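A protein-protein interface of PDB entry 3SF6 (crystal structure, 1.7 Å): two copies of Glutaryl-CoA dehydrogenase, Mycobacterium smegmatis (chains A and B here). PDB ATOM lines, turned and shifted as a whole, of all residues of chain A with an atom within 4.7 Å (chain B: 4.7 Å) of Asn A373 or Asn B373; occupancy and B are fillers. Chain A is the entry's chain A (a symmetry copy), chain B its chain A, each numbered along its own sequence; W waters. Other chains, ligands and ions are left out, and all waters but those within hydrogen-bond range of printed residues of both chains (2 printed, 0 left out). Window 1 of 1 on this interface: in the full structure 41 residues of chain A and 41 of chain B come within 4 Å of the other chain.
Water W2 bridges the side-chain carboxylate of Glu B376 and the side-chain sulfur of Met A369. Water W1 bridges the side-chain carboxylate (OE2) of Glu A376 (2.8 Å) and the side-chain sulfur (SD) of Met B369 (3.6 Å).
Asn A373 touches just these residues of chain B: Met B222, Met B369 and Asn B373. Of the printed residues of chain A, Asn B373 touches Met A222 (3.6 Å), Met A369 (3.4 Å) and Asn A373 (2.9 Å). Of the printed residues of chain A, Arg B370 touches Met A222 (3.6 Å). Printed residues of chain B within 4 Å of Met A369: Met B222 (3.6 Å), Asn B373 (3.4 Å) and Glu B376 (3.9 Å).
Hydrophobic or aromatic side chains of chain A within 4 Å of the printed part of chain B: Tyr A57, Met A222 and Met A369. Of the 12 printed residues of chain B, 6 touch a printed residue of chain A. Printed residues of chain B that touch a printed residue of chain A: Tyr B57, Met B222, Met B369, Arg B370, Asn B373 and Glu B376. Hydrophobic or aromatic side chains of chain B that line the printed part of chain A: Tyr B57, Met B222 and Met B369. Among the printed residues, 13 pairs touch across the chains.
Tyr A57 touches Met B222. Met A222 touches Tyr B57 (CE to CE1, 3.8 Å). O of Met A222 touches CE of Met B369, at 3.6 Å. Met A222 touches Arg B370. Met A369 touches Met B222. Met A369 touches Asn B373 (CE to OD1, 3.4 Å). Glu B376 touches Met A369. Asn A373 touches Met B222 (ND2 to CE, 3.6 Å). Met B369 touches Asn A373. Glu A376 touches Met B369 (CG to SD, 3.9 Å).
Met A222 touches Met B369, and with the chains exchanged Met A369 touches Met B222. Met A222 touches Arg B370, and with the chains exchanged Arg A370 touches Met B222. Met A222 touches Asn B373, and with the chains exchanged Asn A373 touches Met B222. Met A369 touches Asn B373, and with the chains exchanged Asn A373 touches Met B369.
The side-chain amide oxygen (OD1) of Asn B373 lies close to the side-chain amide oxygen (OD1) of Asn A373.
The side-chain amide nitrogen (ND2) of Asn B373 lies close to the backbone carbonyl oxygen (O) of Met B222 (3.5 Å). The side-chain hydroxyl (OG) of Ser B223 is in hydrogen-bond range of the backbone carbonyl oxygen (O) of Asn B373 (2.7 Å). O of Arg B370 sits close to ND2 of Asn B374 (3.3 Å). The side-chain amide nitrogen (ND2) of Asn A373 lies close to the backbone carbonyl oxygen (O) of Met A222 (3.5 Å). The side-chain hydroxyl (OG) of Ser A223 lies within hydrogen-bond range of the backbone carbonyl oxygen (O) of Asn A373 (2.7 Å). The backbone carbonyl oxygen (O) of Arg A370 lies close to the side-chain amide nitrogen (ND2) of Asn A374, 3.3 Å away.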
ATOM      1  N   TYR A  57     -19.977  -3.523  10.281  1.00  0.00           N
ATOM      2  CA  TYR A  57     -18.674  -3.566   9.656  1.00  0.00           C
ATOM      3  C   TYR A  57     -18.740  -4.422   8.353  1.00  0.00           C
ATOM      4  O   TYR A  57     -18.288  -4.020   7.279  1.00  0.00           O
ATOM      5  CB  TYR A  57     -17.621  -4.157  10.603  1.00  0.00           C
ATOM      6  CG  TYR A  57     -16.234  -4.034  10.027  1.00  0.00           C
ATOM      7  CD1 TYR A  57     -15.730  -5.009   9.163  1.00  0.00           C
ATOM      8  CD2 TYR A  57     -15.449  -2.905  10.273  1.00  0.00           C
ATOM      9  CE1 TYR A  57     -14.478  -4.860   8.582  1.00  0.00           C
ATOM     10  CE2 TYR A  57     -14.208  -2.747   9.693  1.00  0.00           C
ATOM     11  CZ  TYR A  57     -13.708  -3.720   8.866  1.00  0.00           C
ATOM     12  OH  TYR A  57     -12.511  -3.603   8.231  1.00  0.00           O
ATOM     13  N   MET A 222     -11.439  -1.602   3.050  1.00  0.00           N
ATOM     14  CA  MET A 222     -10.930  -2.773   3.795  1.00  0.00           C
ATOM     15  C   MET A 222     -10.541  -2.388   5.231  1.00  0.00           C
ATOM     16  O   MET A 222      -9.786  -3.097   5.902  1.00  0.00           O
ATOM     17  CB  MET A 222      -9.751  -3.411   3.032  1.00  0.00           C
ATOM     18  CG  MET A 222     -10.101  -3.863   1.659  1.00  0.00           C
ATOM     19  SD  MET A 222     -10.594  -5.597   1.825  1.00  0.00           S
ATOM     20  CE  MET A 222      -9.133  -6.464   2.312  1.00  0.00           C
ATOM     21  N   SER A 223     -11.035  -1.221   5.664  1.00  0.00           N
ATOM     22  CA  SER A 223     -10.724  -0.623   6.965  1.00  0.00           C
ATOM     23  C   SER A 223     -11.789   0.411   7.242  1.00  0.00           C
ATOM     24  O   SER A 223     -12.299   1.033   6.306  1.00  0.00           O
ATOM     25  CB  SER A 223      -9.373   0.105   6.897  1.00  0.00           C
ATOM     26  OG  SER A 223      -9.112   0.820   8.105  1.00  0.00           O
ATOM     27  N   MET A 369      -9.539  -9.084  13.899  1.00  0.00           N
ATOM     28  CA  MET A 369      -9.274  -8.670  12.540  1.00  0.00           C
ATOM     29  C   MET A 369      -9.929  -7.316  12.253  1.00  0.00           C
ATOM     30  O   MET A 369      -9.340  -6.494  11.527  1.00  0.00           O
ATOM     31  CB  MET A 369      -9.701  -9.718  11.502  1.00  0.00           C
ATOM     32  CG  MET A 369      -8.726 -10.860  11.428  1.00  0.00           C
ATOM     33  SD  MET A 369      -7.121 -10.395  10.807  1.00  0.00           S
ATOM     34  CE  MET A 369      -7.483  -9.653   9.149  1.00  0.00           C
ATOM     35  N   ARG A 370     -11.133  -7.090  12.778  1.00  0.00           N
ATOM     36  CA  ARG A 370     -11.803  -5.775  12.591  1.00  0.00           C
ATOM     37  C   ARG A 370     -10.941  -4.660  13.200  1.00  0.00           C
ATOM     38  O   ARG A 370     -10.691  -3.637  12.563  1.00  0.00           O
ATOM     39  CB  ARG A 370     -13.191  -5.810  13.222  1.00  0.00           C
ATOM     40  CG  ARG A 370     -13.909  -4.469  13.172  1.00  0.00           C
ATOM     41  CD  ARG A 370     -15.385  -4.586  13.478  1.00  0.00           C
ATOM     42  NE  ARG A 370     -15.640  -5.378  14.675  1.00  0.00           N
ATOM     43  CZ  ARG A 370     -15.495  -4.913  15.919  1.00  0.00           C
ATOM     44  NH1 ARG A 370     -15.718  -5.719  16.954  1.00  0.00           N
ATOM     45  NH2 ARG A 370     -15.140  -3.638  16.161  1.00  0.00           N
ATOM     46  N   HIS A 371     -10.509  -4.860  14.439  1.00  0.00           N
ATOM     47  CA  HIS A 371      -9.620  -3.910  15.083  1.00  0.00           C
ATOM     48  C   HIS A 371      -8.326  -3.679  14.294  1.00  0.00           C
ATOM     49  O   HIS A 371      -7.949  -2.520  14.068  1.00  0.00           O
ATOM     50  CB  HIS A 371      -9.268  -4.296  16.511  1.00  0.00           C
ATOM     51  CG  HIS A 371     -10.365  -4.074  17.488  1.00  0.00           C
ATOM     52  ND1 HIS A 371     -11.029  -2.867  17.640  1.00  0.00           N
ATOM     53  CD2 HIS A 371     -10.890  -4.919  18.402  1.00  0.00           C
ATOM     54  CE1 HIS A 371     -11.915  -2.989  18.615  1.00  0.00           C
ATOM     55  NE2 HIS A 371     -11.848  -4.221  19.104  1.00  0.00           N
ATOM     56  N   ALA A 372      -7.668  -4.747  13.857  1.00  0.00           N
ATOM     57  CA  ALA A 372      -6.403  -4.621  13.138  1.00  0.00           C
ATOM     58  C   ALA A 372      -6.618  -3.850  11.821  1.00  0.00           C
ATOM     59  O   ALA A 372      -5.844  -2.955  11.501  1.00  0.00           O
ATOM     60  CB  ALA A 372      -5.788  -6.006  12.870  1.00  0.00           C
ATOM     61  N   ASN A 373      -7.687  -4.174  11.077  1.00  0.00           N
ATOM     62  CA  ASN A 373      -7.938  -3.487   9.832  1.00  0.00           C
ATOM     63  C   ASN A 373      -8.324  -2.017  10.063  1.00  0.00           C
ATOM     64  O   ASN A 373      -7.802  -1.128   9.377  1.00  0.00           O
ATOM     65  CB  ASN A 373      -9.033  -4.196   9.033  1.00  0.00           C
ATOM     66  CG  ASN A 373      -8.533  -5.477   8.326  1.00  0.00           C
ATOM     67  OD1 ASN A 373      -7.341  -5.858   8.396  1.00  0.00           O
ATOM     68  ND2 ASN A 373      -9.435  -6.100   7.598  1.00  0.00           N
ATOM     69  N   ASN A 374      -9.178  -1.760  11.054  1.00  0.00           N
ATOM     70  CA  ASN A 374      -9.517  -0.386  11.436  1.00  0.00           C
ATOM     71  C   ASN A 374      -8.277   0.436  11.759  1.00  0.00           C
ATOM     72  O   ASN A 374      -8.168   1.590  11.343  1.00  0.00           O
ATOM     73  CB  ASN A 374     -10.432  -0.349  12.662  1.00  0.00           C
ATOM     74  CG  ASN A 374     -11.874  -0.662  12.354  1.00  0.00           C
ATOM     75  OD1 ASN A 374     -12.340  -0.533  11.218  1.00  0.00           O
ATOM     76  ND2 ASN A 374     -12.624  -1.069  13.408  1.00  0.00           N
ATOM     77  N   LEU A 375      -7.352  -0.152  12.495  1.00  0.00           N
ATOM     78  CA  LEU A 375      -6.180   0.587  12.930  1.00  0.00           C
ATOM     79  C   LEU A 375      -5.279   0.995  11.797  1.00  0.00           C
ATOM     80  O   LEU A 375      -4.500   1.929  11.954  1.00  0.00           O
ATOM     81  CB  LEU A 375      -5.441  -0.184  14.011  1.00  0.00           C
ATOM     82  CG  LEU A 375      -6.105  -0.165  15.380  1.00  0.00           C
ATOM     83  CD1 LEU A 375      -5.516  -1.256  16.289  1.00  0.00           C
ATOM     84  CD2 LEU A 375      -5.978   1.219  16.085  1.00  0.00           C
ATOM     85  N   GLU A 376      -5.413   0.368  10.621  1.00  0.00           N
ATOM     86  CA  GLU A 376      -4.703   0.878   9.452  1.00  0.00           C
ATOM     87  C   GLU A 376      -5.068   2.340   9.170  1.00  0.00           C
ATOM     88  O   GLU A 376      -4.207   3.173   8.875  1.00  0.00           O
ATOM     89  CB  GLU A 376      -5.003   0.054   8.198  1.00  0.00           C
ATOM     90  CG  GLU A 376      -4.617  -1.401   8.242  1.00  0.00           C
ATOM     91  CD  GLU A 376      -3.156  -1.688   8.048  1.00  0.00           C
ATOM     92  OE1 GLU A 376      -2.376  -0.767   7.703  1.00  0.00           O
ATOM     93  OE2 GLU A 376      -2.828  -2.881   8.283  1.00  0.00           O
ATOM     94  N   SER A 377      -6.365   2.676   9.236  1.00  0.00           N
ATOM     95  CA  SER A 377      -6.788   4.058   8.992  1.00  0.00           C
ATOM     96  C   SER A 377      -6.299   4.974  10.090  1.00  0.00           C
ATOM     97  O   SER A 377      -5.861   6.089   9.822  1.00  0.00           O
ATOM     98  CB  SER A 377      -8.309   4.140   8.905  1.00  0.00           C
ATOM     99  OG  SER A 377      -8.776   3.491   7.729  1.00  0.00           O
ATOM    100  N   TYR B  57     -13.319 -11.452  -3.852  1.00  0.00           N
ATOM    101  CA  TYR B  57     -12.898 -11.296  -2.477  1.00  0.00           C
ATOM    102  C   TYR B  57     -13.985 -10.516  -1.675  1.00  0.00           C
ATOM    103  O   TYR B  57     -14.417 -10.917  -0.592  1.00  0.00           O
ATOM    104  CB  TYR B  57     -11.561 -10.546  -2.387  1.00  0.00           C
ATOM    105  CG  TYR B  57     -11.027 -10.543  -0.978  1.00  0.00           C
ATOM    106  CD1 TYR B  57     -11.423  -9.561  -0.068  1.00  0.00           C
ATOM    107  CD2 TYR B  57     -10.192 -11.565  -0.521  1.00  0.00           C
ATOM    108  CE1 TYR B  57     -10.982  -9.598   1.249  1.00  0.00           C
ATOM    109  CE2 TYR B  57      -9.757 -11.612   0.786  1.00  0.00           C
ATOM    110  CZ  TYR B  57     -10.128 -10.630   1.669  1.00  0.00           C
ATOM    111  OH  TYR B  57      -9.767 -10.645   2.981  1.00  0.00           O
ATOM    112  N   MET B 222     -12.590 -12.762   7.402  1.00  0.00           N
ATOM    113  CA  MET B 222     -11.833 -11.507   7.206  1.00  0.00           C
ATOM    114  C   MET B 222     -10.483 -11.776   6.526  1.00  0.00           C
ATOM    115  O   MET B 222      -9.562 -10.958   6.581  1.00  0.00           O
ATOM    116  CB  MET B 222     -11.661 -10.780   8.555  1.00  0.00           C
ATOM    117  CG  MET B 222     -12.948 -10.435   9.218  1.00  0.00           C
ATOM    118  SD  MET B 222     -13.353  -8.761   8.662  1.00  0.00           S
ATOM    119  CE  MET B 222     -12.106  -7.715   9.351  1.00  0.00           C
ATOM    120  N   SER B 223     -10.373 -12.969   5.925  1.00  0.00           N
ATOM    121  CA  SER B 223      -9.149 -13.466   5.290  1.00  0.00           C
ATOM    122  C   SER B 223      -9.553 -14.597   4.376  1.00  0.00           C
ATOM    123  O   SER B 223     -10.511 -15.316   4.675  1.00  0.00           O
ATOM    124  CB  SER B 223      -8.204 -14.042   6.356  1.00  0.00           C
ATOM    125  OG  SER B 223      -7.068 -14.665   5.753  1.00  0.00           O
ATOM    126  N   MET B 369      -4.238  -4.603   1.002  1.00  0.00           N
ATOM    127  CA  MET B 369      -5.001  -5.049   2.145  1.00  0.00           C
ATOM    128  C   MET B 369      -5.504  -6.480   1.930  1.00  0.00           C
ATOM    129  O   MET B 369      -5.542  -7.265   2.895  1.00  0.00           O
ATOM    130  CB  MET B 369      -6.162  -4.106   2.494  1.00  0.00           C
ATOM    131  CG  MET B 369      -5.683  -2.868   3.199  1.00  0.00           C
ATOM    132  SD  MET B 369      -4.996  -3.181   4.815  1.00  0.00           S
ATOM    133  CE  MET B 369      -6.366  -4.038   5.721  1.00  0.00           C
ATOM    134  N   ARG B 370      -5.911  -6.812   0.706  1.00  0.00           N
ATOM    135  CA  ARG B 370      -6.356  -8.200   0.409  1.00  0.00           C
ATOM    136  C   ARG B 370      -5.206  -9.183   0.673  1.00  0.00           C
ATOM    137  O   ARG B 370      -5.386 -10.201   1.340  1.00  0.00           O
ATOM    138  CB  ARG B 370      -6.839  -8.289  -1.035  1.00  0.00           C
ATOM    139  CG  ARG B 370      -7.214  -9.702  -1.459  1.00  0.00           C
ATOM    140  CD  ARG B 370      -8.003  -9.735  -2.748  1.00  0.00           C
ATOM    141  NE  ARG B 370      -7.391  -8.919  -3.790  1.00  0.00           N
ATOM    142  CZ  ARG B 370      -6.337  -9.305  -4.513  1.00  0.00           C
ATOM    143  NH1 ARG B 370      -5.823  -8.480  -5.423  1.00  0.00           N
ATOM    144  NH2 ARG B 370      -5.779 -10.520  -4.359  1.00  0.00           N
ATOM    145  N   HIS B 371      -4.033  -8.876   0.130  1.00  0.00           N
ATOM    146  CA  HIS B 371      -2.857  -9.690   0.382  1.00  0.00           C
ATOM    147  C   HIS B 371      -2.531  -9.815   1.875  1.00  0.00           C
ATOM    148  O   HIS B 371      -2.312 -10.934   2.360  1.00  0.00           O
ATOM    149  CB  HIS B 371      -1.623  -9.200  -0.357  1.00  0.00           C
ATOM    150  CG  HIS B 371      -1.630  -9.495  -1.813  1.00  0.00           C
ATOM    151  ND1 HIS B 371      -1.835 -10.759  -2.343  1.00  0.00           N
ATOM    152  CD2 HIS B 371      -1.414  -8.669  -2.861  1.00  0.00           C
ATOM    153  CE1 HIS B 371      -1.738 -10.689  -3.660  1.00  0.00           C
ATOM    154  NE2 HIS B 371      -1.474  -9.435  -4.005  1.00  0.00           N
ATOM    155  N   ALA B 372      -2.521  -8.702   2.602  1.00  0.00           N
ATOM    156  CA  ALA B 372      -2.175  -8.722   4.020  1.00  0.00           C
ATOM    157  C   ALA B 372      -3.194  -9.574   4.802  1.00  0.00           C
ATOM    158  O   ALA B 372      -2.804 -10.392   5.627  1.00  0.00           O
ATOM    159  CB  ALA B 372      -2.107  -7.292   4.585  1.00  0.00           C
ATOM    160  N   ASN B 373      -4.494  -9.407   4.517  1.00  0.00           N
ATOM    161  CA  ASN B 373      -5.494 -10.176   5.219  1.00  0.00           C
ATOM    162  C   ASN B 373      -5.425 -11.667   4.851  1.00  0.00           C
ATOM    163  O   ASN B 373      -5.472 -12.525   5.744  1.00  0.00           O
ATOM    164  CB  ASN B 373      -6.895  -9.632   4.935  1.00  0.00           C
ATOM    165  CG  ASN B 373      -7.214  -8.339   5.721  1.00  0.00           C
ATOM    166  OD1 ASN B 373      -6.398  -7.826   6.522  1.00  0.00           O
ATOM    167  ND2 ASN B 373      -8.422  -7.856   5.532  1.00  0.00           N
ATOM    168  N   ASN B 374      -5.253 -11.969   3.564  1.00  0.00           N
ATOM    169  CA  ASN B 374      -5.052 -13.352   3.122  1.00  0.00           C
ATOM    170  C   ASN B 374      -3.886 -14.015   3.842  1.00  0.00           C
ATOM    171  O   ASN B 374      -3.987 -15.169   4.262  1.00  0.00           O
ATOM    172  CB  ASN B 374      -4.775 -13.432   1.619  1.00  0.00           C
ATOM    173  CG  ASN B 374      -6.009 -13.296   0.765  1.00  0.00           C
ATOM    174  OD1 ASN B 374      -7.137 -13.529   1.209  1.00  0.00           O
ATOM    175  ND2 ASN B 374      -5.795 -12.924  -0.522  1.00  0.00           N
ATOM    176  N   LEU B 375      -2.789 -13.294   3.984  1.00  0.00           N
ATOM    177  CA  LEU B 375      -1.598 -13.877   4.575  1.00  0.00           C
ATOM    178  C   LEU B 375      -1.768 -14.236   6.026  1.00  0.00           C
ATOM    179  O   LEU B 375      -1.023 -15.070   6.530  1.00  0.00           O
ATOM    180  CB  LEU B 375      -0.397 -12.978   4.336  1.00  0.00           C
ATOM    181  CG  LEU B 375       0.152 -13.005   2.917  1.00  0.00           C
ATOM    182  CD1 LEU B 375       1.092 -11.812   2.672  1.00  0.00           C
ATOM    183  CD2 LEU B 375       0.905 -14.330   2.594  1.00  0.00           C
ATOM    184  N   GLU B 376      -2.784 -13.686   6.703  1.00  0.00           N
ATOM    185  CA  GLU B 376      -3.098 -14.170   8.044  1.00  0.00           C
ATOM    186  C   GLU B 376      -3.388 -15.675   8.041  1.00  0.00           C
ATOM    187  O   GLU B 376      -2.928 -16.421   8.909  1.00  0.00           O
ATOM    188  CB  GLU B 376      -4.304 -13.445   8.644  1.00  0.00           C
ATOM    189  CG  GLU B 376      -4.173 -11.956   8.824  1.00  0.00           C
ATOM    190  CD  GLU B 376      -3.357 -11.518  10.007  1.00  0.00           C
ATOM    191  OE1 GLU B 376      -2.978 -12.363  10.854  1.00  0.00           O
ATOM    192  OE2 GLU B 376      -3.096 -10.286  10.027  1.00  0.00           O
ATOM    193  N   SER B 377      -4.181 -16.148   7.068  1.00  0.00           N
ATOM    194  CA  SER B 377      -4.491 -17.579   6.993  1.00  0.00           C
ATOM    195  C   SER B 377      -3.260 -18.382   6.643  1.00  0.00           C
ATOM    196  O   SER B 377      -3.035 -19.453   7.198  1.00  0.00           O
ATOM    197  CB  SER B 377      -5.575 -17.833   5.950  1.00  0.00           C
ATOM    198  OG  SER B 377      -6.819 -17.298   6.383  1.00  0.00           O
HETATM  199  O   HOH W   1      -1.936  -4.436   6.186  1.00  0.00           O
HETATM  200  O   HOH W   2      -4.191  -8.745  12.036  1.00  0.00           O
